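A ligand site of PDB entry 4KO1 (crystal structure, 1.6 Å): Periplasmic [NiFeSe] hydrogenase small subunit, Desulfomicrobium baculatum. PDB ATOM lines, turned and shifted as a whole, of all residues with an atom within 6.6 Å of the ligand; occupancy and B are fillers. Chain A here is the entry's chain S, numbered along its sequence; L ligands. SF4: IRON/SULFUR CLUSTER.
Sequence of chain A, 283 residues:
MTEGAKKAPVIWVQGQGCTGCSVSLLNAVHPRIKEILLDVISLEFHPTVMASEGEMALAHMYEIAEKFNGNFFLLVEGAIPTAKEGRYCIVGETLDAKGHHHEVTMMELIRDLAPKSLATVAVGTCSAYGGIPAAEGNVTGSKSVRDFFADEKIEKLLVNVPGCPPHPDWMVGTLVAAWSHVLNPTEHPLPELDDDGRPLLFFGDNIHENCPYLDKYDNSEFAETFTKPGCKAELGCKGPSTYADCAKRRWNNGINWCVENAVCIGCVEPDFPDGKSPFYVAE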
ATOM      1  N   ILE A 207       6.540  21.995 -31.864  1.00  0.00           N
ATOM      2  CA  ILE A 207       7.219  20.750 -32.259  1.00  0.00           C
ATOM      3  C   ILE A 207       7.733  20.028 -31.014  1.00  0.00           C
ATOM      4  O   ILE A 207       7.444  18.847 -30.809  1.00  0.00           O
ATOM      5  CB  ILE A 207       8.391  21.022 -33.242  1.00  0.00           C
ATOM      6  CG1 ILE A 207       7.887  21.620 -34.580  1.00  0.00           C
ATOM      7  CG2 ILE A 207       9.283  19.761 -33.431  1.00  0.00           C
ATOM      8  CD1 ILE A 207       7.689  20.655 -35.715  1.00  0.00           C
ATOM      9  N   HIS A 208       8.482  20.740 -30.173  1.00  0.00           N
ATOM     10  CA  HIS A 208       9.118  20.163 -28.993  1.00  0.00           C
ATOM     11  C   HIS A 208       8.097  19.517 -28.032  1.00  0.00           C
ATOM     12  O   HIS A 208       8.265  18.363 -27.616  1.00  0.00           O
ATOM     13  CB  HIS A 208       9.975  21.256 -28.336  1.00  0.00           C
ATOM     14  CG  HIS A 208      10.622  20.869 -27.056  1.00  0.00           C
ATOM     15  ND1 HIS A 208      11.742  20.069 -26.990  1.00  0.00           N
ATOM     16  CD2 HIS A 208      10.349  21.251 -25.777  1.00  0.00           C
ATOM     17  CE1 HIS A 208      12.108  19.937 -25.717  1.00  0.00           C
ATOM     18  NE2 HIS A 208      11.284  20.639 -24.969  1.00  0.00           N
ATOM     19  N   GLU A 209       7.007  20.227 -27.734  1.00  0.00           N
ATOM     20  CA  GLU A 209       5.959  19.715 -26.834  1.00  0.00           C
ATOM     21  C   GLU A 209       5.362  18.417 -27.362  1.00  0.00           C
ATOM     22  O   GLU A 209       4.890  17.573 -26.587  1.00  0.00           O
ATOM     23  CB  GLU A 209       4.867  20.760 -26.617  1.00  0.00           C
ATOM     24  CG  GLU A 209       5.310  21.982 -25.804  1.00  0.00           C
ATOM     25  CD  GLU A 209       4.244  23.063 -25.686  1.00  0.00           C
ATOM     26  OE1 GLU A 209       3.038  22.792 -25.920  1.00  0.00           O
ATOM     27  OE2 GLU A 209       4.607  24.209 -25.356  1.00  0.00           O
ATOM     28  N   CYS A 211       7.095  16.249 -29.416  1.00  0.00           N
ATOM     29  CA  CYS A 211       8.182  15.457 -29.972  1.00  0.00           C
ATOM     30  C   CYS A 211       8.303  14.090 -29.295  1.00  0.00           C
ATOM     31  O   CYS A 211       8.242  13.996 -28.066  1.00  0.00           O
ATOM     32  CB  CYS A 211       9.490  16.206 -29.821  1.00  0.00           C
ATOM     33  SG  CYS A 211      10.872  15.364 -30.584  1.00  0.00           S
ATOM     34  N   PRO A 212       8.513  13.028 -30.087  1.00  0.00           N
ATOM     35  CA  PRO A 212       8.732  11.712 -29.451  1.00  0.00           C
ATOM     36  C   PRO A 212      10.036  11.595 -28.637  1.00  0.00           C
ATOM     37  O   PRO A 212      10.207  10.614 -27.901  1.00  0.00           O
ATOM     38  CB  PRO A 212       8.766  10.752 -30.642  1.00  0.00           C
ATOM     39  CG  PRO A 212       9.118  11.597 -31.821  1.00  0.00           C
ATOM     40  CD  PRO A 212       8.483  12.943 -31.559  1.00  0.00           C
ATOM     41  N   TYR A 213      10.947  12.560 -28.777  1.00  0.00           N
ATOM     42  CA  TYR A 213      12.200  12.550 -28.002  1.00  0.00           C
ATOM     43  C   TYR A 213      12.063  13.291 -26.687  1.00  0.00           C
ATOM     44  O   TYR A 213      13.048  13.416 -25.961  1.00  0.00           O
ATOM     45  CB  TYR A 213      13.353  13.181 -28.787  1.00  0.00           C
ATOM     46  CG  TYR A 213      13.821  12.398 -29.993  1.00  0.00           C
ATOM     47  CD1 TYR A 213      13.217  12.562 -31.233  1.00  0.00           C
ATOM     48  CD2 TYR A 213      14.904  11.506 -29.893  1.00  0.00           C
ATOM     49  CE1 TYR A 213      13.653  11.852 -32.349  1.00  0.00           C
ATOM     50  CE2 TYR A 213      15.347  10.791 -31.006  1.00  0.00           C
ATOM     51  CZ  TYR A 213      14.714  10.972 -32.232  1.00  0.00           C
ATOM     52  OH  TYR A 213      15.141  10.272 -33.340  1.00  0.00           O
ATOM     53  N   LEU A 214      10.868  13.808 -26.380  1.00  0.00           N
ATOM     54  CA  LEU A 214      10.706  14.642 -25.195  1.00  0.00           C
ATOM     55  C   LEU A 214      11.055  13.901 -23.899  1.00  0.00           C
ATOM     56  O   LEU A 214      11.628  14.495 -23.003  1.00  0.00           O
ATOM     57  CB  LEU A 214       9.290  15.237 -25.130  1.00  0.00           C
ATOM     58  CG  LEU A 214       9.069  16.327 -24.072  1.00  0.00           C
ATOM     59  CD1 LEU A 214       9.935  17.540 -24.367  1.00  0.00           C
ATOM     60  CD2 LEU A 214       7.592  16.716 -24.004  1.00  0.00           C
ATOM     61  N   ASP A 215      10.760  12.596 -23.819  1.00  0.00           N
ATOM     62  CA  ASP A 215      11.145  11.791 -22.648  1.00  0.00           C
ATOM     63  C   ASP A 215      12.675  11.781 -22.451  1.00  0.00           C
ATOM     64  O   ASP A 215      13.175  11.898 -21.335  1.00  0.00           O
ATOM     65  CB  ASP A 215      10.592  10.352 -22.772  1.00  0.00           C
ATOM     66  CG  ASP A 215      11.153   9.573 -23.980  1.00  0.00           C
ATOM     67  OD1 ASP A 215      11.489  10.179 -25.039  1.00  0.00           O
ATOM     68  OD2 ASP A 215      11.237   8.328 -23.882  1.00  0.00           O
ATOM     69  N   LYS A 216      13.407  11.699 -23.545  1.00  0.00           N
ATOM     70  CA  LYS A 216      14.859  11.731 -23.513  1.00  0.00           C
ATOM     71  C   LYS A 216      15.376  13.115 -23.112  1.00  0.00           C
ATOM     72  O   LYS A 216      16.295  13.236 -22.288  1.00  0.00           O
ATOM     73  CB  LYS A 216      15.420  11.300 -24.870  1.00  0.00           C
ATOM     74  CG  LYS A 216      15.320   9.787 -25.098  1.00  0.00           C
ATOM     75  CD  LYS A 216      15.262   9.424 -26.552  1.00  0.00           C
ATOM     76  CE  LYS A 216      14.990   7.931 -26.744  1.00  0.00           C
ATOM     77  NZ  LYS A 216      14.614   7.610 -28.169  1.00  0.00           N
ATOM     78  N   TYR A 217      14.793  14.159 -23.687  1.00  0.00           N
ATOM     79  CA  TYR A 217      15.103  15.538 -23.283  1.00  0.00           C
ATOM     80  C   TYR A 217      14.939  15.704 -21.765  1.00  0.00           C
ATOM     81  O   TYR A 217      15.811  16.265 -21.093  1.00  0.00           O
ATOM     82  CB  TYR A 217      14.178  16.505 -24.020  1.00  0.00           C
ATOM     83  CG  TYR A 217      14.338  17.956 -23.610  1.00  0.00           C
ATOM     84  CD1 TYR A 217      13.570  18.486 -22.586  1.00  0.00           C
ATOM     85  CD2 TYR A 217      15.244  18.794 -24.278  1.00  0.00           C
ATOM     86  CE1 TYR A 217      13.706  19.827 -22.198  1.00  0.00           C
ATOM     87  CE2 TYR A 217      15.377  20.141 -23.914  1.00  0.00           C
ATOM     88  CZ  TYR A 217      14.607  20.641 -22.868  1.00  0.00           C
ATOM     89  OH  TYR A 217      14.731  21.956 -22.504  1.00  0.00           O
ATOM     90  N   PHE A 222      20.984  13.348 -24.331  1.00  0.00           N
ATOM     91  CA  PHE A 222      21.216  14.101 -25.550  1.00  0.00           C
ATOM     92  C   PHE A 222      22.191  13.372 -26.470  1.00  0.00           C
ATOM     93  O   PHE A 222      23.242  12.891 -26.031  1.00  0.00           O
ATOM     94  CB  PHE A 222      21.756  15.490 -25.226  1.00  0.00           C
ATOM     95  CG  PHE A 222      20.814  16.319 -24.397  1.00  0.00           C
ATOM     96  CD1 PHE A 222      19.617  16.789 -24.937  1.00  0.00           C
ATOM     97  CD2 PHE A 222      21.105  16.595 -23.062  1.00  0.00           C
ATOM     98  CE1 PHE A 222      18.742  17.561 -24.184  1.00  0.00           C
ATOM     99  CE2 PHE A 222      20.246  17.360 -22.294  1.00  0.00           C
ATOM    100  CZ  PHE A 222      19.048  17.839 -22.849  1.00  0.00           C
ATOM    101  N   GLY A 230      19.357   9.698 -28.386  1.00  0.00           N
ATOM    102  CA  GLY A 230      19.041  10.838 -27.548  1.00  0.00           C
ATOM    103  C   GLY A 230      18.312  11.960 -28.269  1.00  0.00           C
ATOM    104  O   GLY A 230      18.219  11.977 -29.501  1.00  0.00           O
ATOM    105  N   CYS A 231      17.811  12.895 -27.482  1.00  0.00           N
ATOM    106  CA  CYS A 231      17.243  14.150 -27.965  1.00  0.00           C
ATOM    107  C   CYS A 231      18.299  14.914 -28.788  1.00  0.00           C
ATOM    108  O   CYS A 231      19.507  14.839 -28.501  1.00  0.00           O
ATOM    109  CB  CYS A 231      16.749  14.968 -26.761  1.00  0.00           C
ATOM    110  SG  CYS A 231      16.535  16.732 -27.051  1.00  0.00           S
ATOM    111  N   LYS A 232      17.838  15.658 -29.787  1.00  0.00           N
ATOM    112  CA  LYS A 232      18.717  16.359 -30.734  1.00  0.00           C
ATOM    113  C   LYS A 232      19.079  17.798 -30.310  1.00  0.00           C
ATOM    114  O   LYS A 232      19.721  18.525 -31.096  1.00  0.00           O
ATOM    115  CB  LYS A 232      18.076  16.415 -32.127  1.00  0.00           C
ATOM    116  CG  LYS A 232      17.512  15.081 -32.642  1.00  0.00           C
ATOM    117  CD  LYS A 232      18.602  14.001 -32.707  1.00  0.00           C
ATOM    118  CE  LYS A 232      18.117  12.784 -33.490  1.00  0.00           C
ATOM    119  NZ  LYS A 232      18.039  13.053 -34.954  1.00  0.00           N
ATOM    120  N   ALA A 233      18.707  18.197 -29.091  1.00  0.00           N
ATOM    121  CA  ALA A 233      18.880  19.596 -28.683  1.00  0.00           C
ATOM    122  C   ALA A 233      20.309  20.104 -28.837  1.00  0.00           C
ATOM    123  O   ALA A 233      20.534  21.217 -29.326  1.00  0.00           O
ATOM    124  CB  ALA A 233      18.395  19.803 -27.221  1.00  0.00           C
ATOM    125  N   GLU A 234      21.291  19.305 -28.387  1.00  0.00           N
ATOM    126  CA  GLU A 234      22.683  19.749 -28.432  1.00  0.00           C
ATOM    127  C   GLU A 234      23.246  19.807 -29.844  1.00  0.00           C
ATOM    128  O   GLU A 234      24.293  20.432 -30.050  1.00  0.00           O
ATOM    129  CB  GLU A 234      23.583  18.871 -27.547  1.00  0.00           C
ATOM    130  CG  GLU A 234      23.292  18.958 -26.052  1.00  0.00           C
ATOM    131  CD  GLU A 234      24.193  18.043 -25.228  1.00  0.00           C
ATOM    132  OE1 GLU A 234      24.100  18.103 -23.980  1.00  0.00           O
ATOM    133  OE2 GLU A 234      24.978  17.261 -25.807  1.00  0.00           O
ATOM    134  N   CYS A 237      18.818  21.430 -32.541  1.00  0.00           N
ATOM    135  CA  CYS A 237      17.369  21.342 -32.787  1.00  0.00           C
ATOM    136  C   CYS A 237      16.596  22.606 -32.366  1.00  0.00           C
ATOM    137  O   CYS A 237      16.713  23.064 -31.214  1.00  0.00           O
ATOM    138  CB  CYS A 237      16.776  20.102 -32.110  1.00  0.00           C
ATOM    139  SG  CYS A 237      15.077  19.800 -32.574  1.00  0.00           S
ATOM    140  N   LYS A 238      15.810  23.171 -33.296  1.00  0.00           N
ATOM    141  CA  LYS A 238      15.005  24.346 -33.001  1.00  0.00           C
ATOM    142  C   LYS A 238      13.539  24.024 -32.723  1.00  0.00           C
ATOM    143  O   LYS A 238      12.685  24.922 -32.667  1.00  0.00           O
ATOM    144  CB  LYS A 238      15.111  25.417 -34.113  1.00  0.00           C
ATOM    145  CG  LYS A 238      16.564  25.835 -34.416  1.00  0.00           C
ATOM    146  CD  LYS A 238      17.304  26.273 -33.143  1.00  0.00           C
ATOM    147  CE  LYS A 238      18.674  26.909 -33.441  1.00  0.00           C
ATOM    148  NZ  LYS A 238      19.524  26.055 -34.324  1.00  0.00           N
ATOM    149  N   GLY A 239      13.241  22.741 -32.523  1.00  0.00           N
ATOM    150  CA  GLY A 239      11.900  22.317 -32.134  1.00  0.00           C
ATOM    151  C   GLY A 239      11.282  23.129 -31.001  1.00  0.00           C
ATOM    152  O   GLY A 239      10.081  23.419 -31.059  1.00  0.00           O
ATOM    153  N   PRO A 240      12.078  23.476 -29.951  1.00  0.00           N
ATOM    154  CA  PRO A 240      11.513  24.251 -28.838  1.00  0.00           C
ATOM    155  C   PRO A 240      10.876  25.582 -29.232  1.00  0.00           C
ATOM    156  O   PRO A 240       9.944  26.025 -28.547  1.00  0.00           O
ATOM    157  CB  PRO A 240      12.733  24.457 -27.919  1.00  0.00           C
ATOM    158  CG  PRO A 240      13.531  23.191 -28.148  1.00  0.00           C
ATOM    159  CD  PRO A 240      13.436  22.994 -29.631  1.00  0.00           C
ATOM    160  N   TRP A 257      11.130  12.462 -40.932  1.00  0.00           N
ATOM    161  CA  TRP A 257      10.991  13.898 -40.674  1.00  0.00           C
ATOM    162  C   TRP A 257      12.287  14.449 -40.108  1.00  0.00           C
ATOM    163  O   TRP A 257      13.204  13.674 -39.773  1.00  0.00           O
ATOM    164  CB  TRP A 257       9.785  14.229 -39.776  1.00  0.00           C
ATOM    165  CG  TRP A 257       9.903  13.801 -38.328  1.00  0.00           C
ATOM    166  CD1 TRP A 257      10.103  12.525 -37.845  1.00  0.00           C
ATOM    167  CD2 TRP A 257       9.724  14.649 -37.180  1.00  0.00           C
ATOM    168  NE1 TRP A 257      10.086  12.546 -36.466  1.00  0.00           N
ATOM    169  CE2 TRP A 257       9.867  13.830 -36.035  1.00  0.00           C
ATOM    170  CE3 TRP A 257       9.482  16.015 -37.013  1.00  0.00           C
ATOM    171  CZ2 TRP A 257       9.751  14.339 -34.719  1.00  0.00           C
ATOM    172  CZ3 TRP A 257       9.370  16.537 -35.724  1.00  0.00           C
ATOM    173  CH2 TRP A 257       9.517  15.686 -34.587  1.00  0.00           C
ATOM    174  N   VAL A 259      13.452  15.911 -37.436  1.00  0.00           N
ATOM    175  CA  VAL A 259      13.944  15.648 -36.094  1.00  0.00           C
ATOM    176  C   VAL A 259      14.440  14.209 -35.937  1.00  0.00           C
ATOM    177  O   VAL A 259      15.494  13.991 -35.361  1.00  0.00           O
ATOM    178  CB  VAL A 259      12.892  16.010 -35.027  1.00  0.00           C
ATOM    179  CG1 VAL A 259      13.296  15.505 -33.626  1.00  0.00           C
ATOM    180  CG2 VAL A 259      12.638  17.527 -35.023  1.00  0.00           C
ATOM    181  N   ALA A 262      17.668  14.228 -38.193  1.00  0.00           N
ATOM    182  CA  ALA A 262      18.725  15.209 -37.934  1.00  0.00           C
ATOM    183  C   ALA A 262      18.265  16.210 -36.884  1.00  0.00           C
ATOM    184  O   ALA A 262      18.194  15.866 -35.732  1.00  0.00           O
ATOM    185  CB  ALA A 262      19.158  15.915 -39.233  1.00  0.00           C
ATOM    186  N   VAL A 263      17.946  17.433 -37.303  1.00  0.00           N
ATOM    187  CA  VAL A 263      17.417  18.474 -36.406  1.00  0.00           C
ATOM    188  C   VAL A 263      16.316  19.258 -37.117  1.00  0.00           C
ATOM    189  O   VAL A 263      16.287  19.327 -38.358  1.00  0.00           O
ATOM    190  CB  VAL A 263      18.521  19.493 -35.980  1.00  0.00           C
ATOM    191  CG1 VAL A 263      19.554  18.844 -35.020  1.00  0.00           C
ATOM    192  CG2 VAL A 263      19.225  20.111 -37.205  1.00  0.00           C
ATOM    193  N   CYS A 264      15.408  19.843 -36.325  1.00  0.00           N
ATOM    194  CA  CYS A 264      14.509  20.876 -36.831  1.00  0.00           C
ATOM    195  C   CYS A 264      15.306  22.180 -36.999  1.00  0.00           C
ATOM    196  O   CYS A 264      16.090  22.557 -36.109  1.00  0.00           O
ATOM    197  CB  CYS A 264      13.333  21.104 -35.852  1.00  0.00           C
ATOM    198  SG  CYS A 264      12.177  22.425 -36.367  1.00  0.00           S
HETATM  199 FE1  SF4 L   1      14.754  17.221 -28.385  1.00  0.00          FE
HETATM  200 FE2  SF4 L   1      12.512  16.790 -29.875  1.00  0.00          FE
HETATM  201 FE3  SF4 L   1      12.778  18.979 -28.416  1.00  0.00          FE
HETATM  202 FE4  SF4 L   1      14.285  18.705 -30.692  1.00  0.00          FE
HETATM  203  S1  SF4 L   1      12.004  18.927 -30.568  1.00  0.00           S
HETATM  204  S2  SF4 L   1      14.997  19.504 -28.699  1.00  0.00           S
HETATM  205  S3  SF4 L   1      14.684  16.429 -30.501  1.00  0.00           S
HETATM  206  S4  SF4 L   1      12.665  16.833 -27.598  1.00  0.00           S
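A ring nitrogen (ND1) of His 208 binds an iron atom (FE3) of the ligand (2.1 Å).
An iron atom (FE1) of the ligand is bound by the side-chain sulfur of Cys 231, at 2.3 Å.
The side-chain sulfur (SG) of Cys 211 is bound to an iron atom (FE2) of the ligand, 2.3 Å away.
The side-chain sulfur (SG) of Cys 237 is bound to an iron atom (FE4) of the ligand (2.3 Å).
The backbone NH (N) of Lys 232 sits close to a sulfur (S3) of the ligand.
The backbone NH (N) of Leu 214 sits close to a sulfur (S4) of the ligand.
Merely in contact with the ligand: Tyr 213 (3.7 Å), Tyr 217 (3.9 Å), Ala 233 (3.7 Å), Gly 239 (3.7 Å), Pro 240 (3.9 Å) and Val 259 (3.5 Å).
Hydrophobic or aromatic side chains that line the ligand: His 208, Tyr 213, Tyr 217, Ala 233, Pro 240 and Val 259.
Of the 25 residues printed, 12 come within 4 Å of the ligand.
The nearest printed residue that does not touch the ligand is Ile 207 (4.04 Å).
O of Gly 239 lies within hydrogen-bond range of N of His 208 (3.2 Å).
The side-chain sulfur of Cys 231 lies close to the backbone NH of Ala 233 (3.3 Å).
The backbone NH of Tyr 213 lies close to the side-chain sulfur of Cys 211, 3.3 Å away.
The backbone NH of Cys 237 is in hydrogen-bond range of the backbone carbonyl oxygen of Lys 232, 3.4 Å away.
The side-chain sulfur (SG) of Cys 237 sits close to the backbone NH (N) of Gly 239, at 3.5 Å.
The side-chain sulfur (SG) of Cys 237 lies close to the backbone NH (N) of Cys 264 (3.8 Å).
O of Val 259 lies within hydrogen-bond range of NZ of Lys 232.
NZ of Lys 232 lies within hydrogen-bond range of O of Ala 262.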
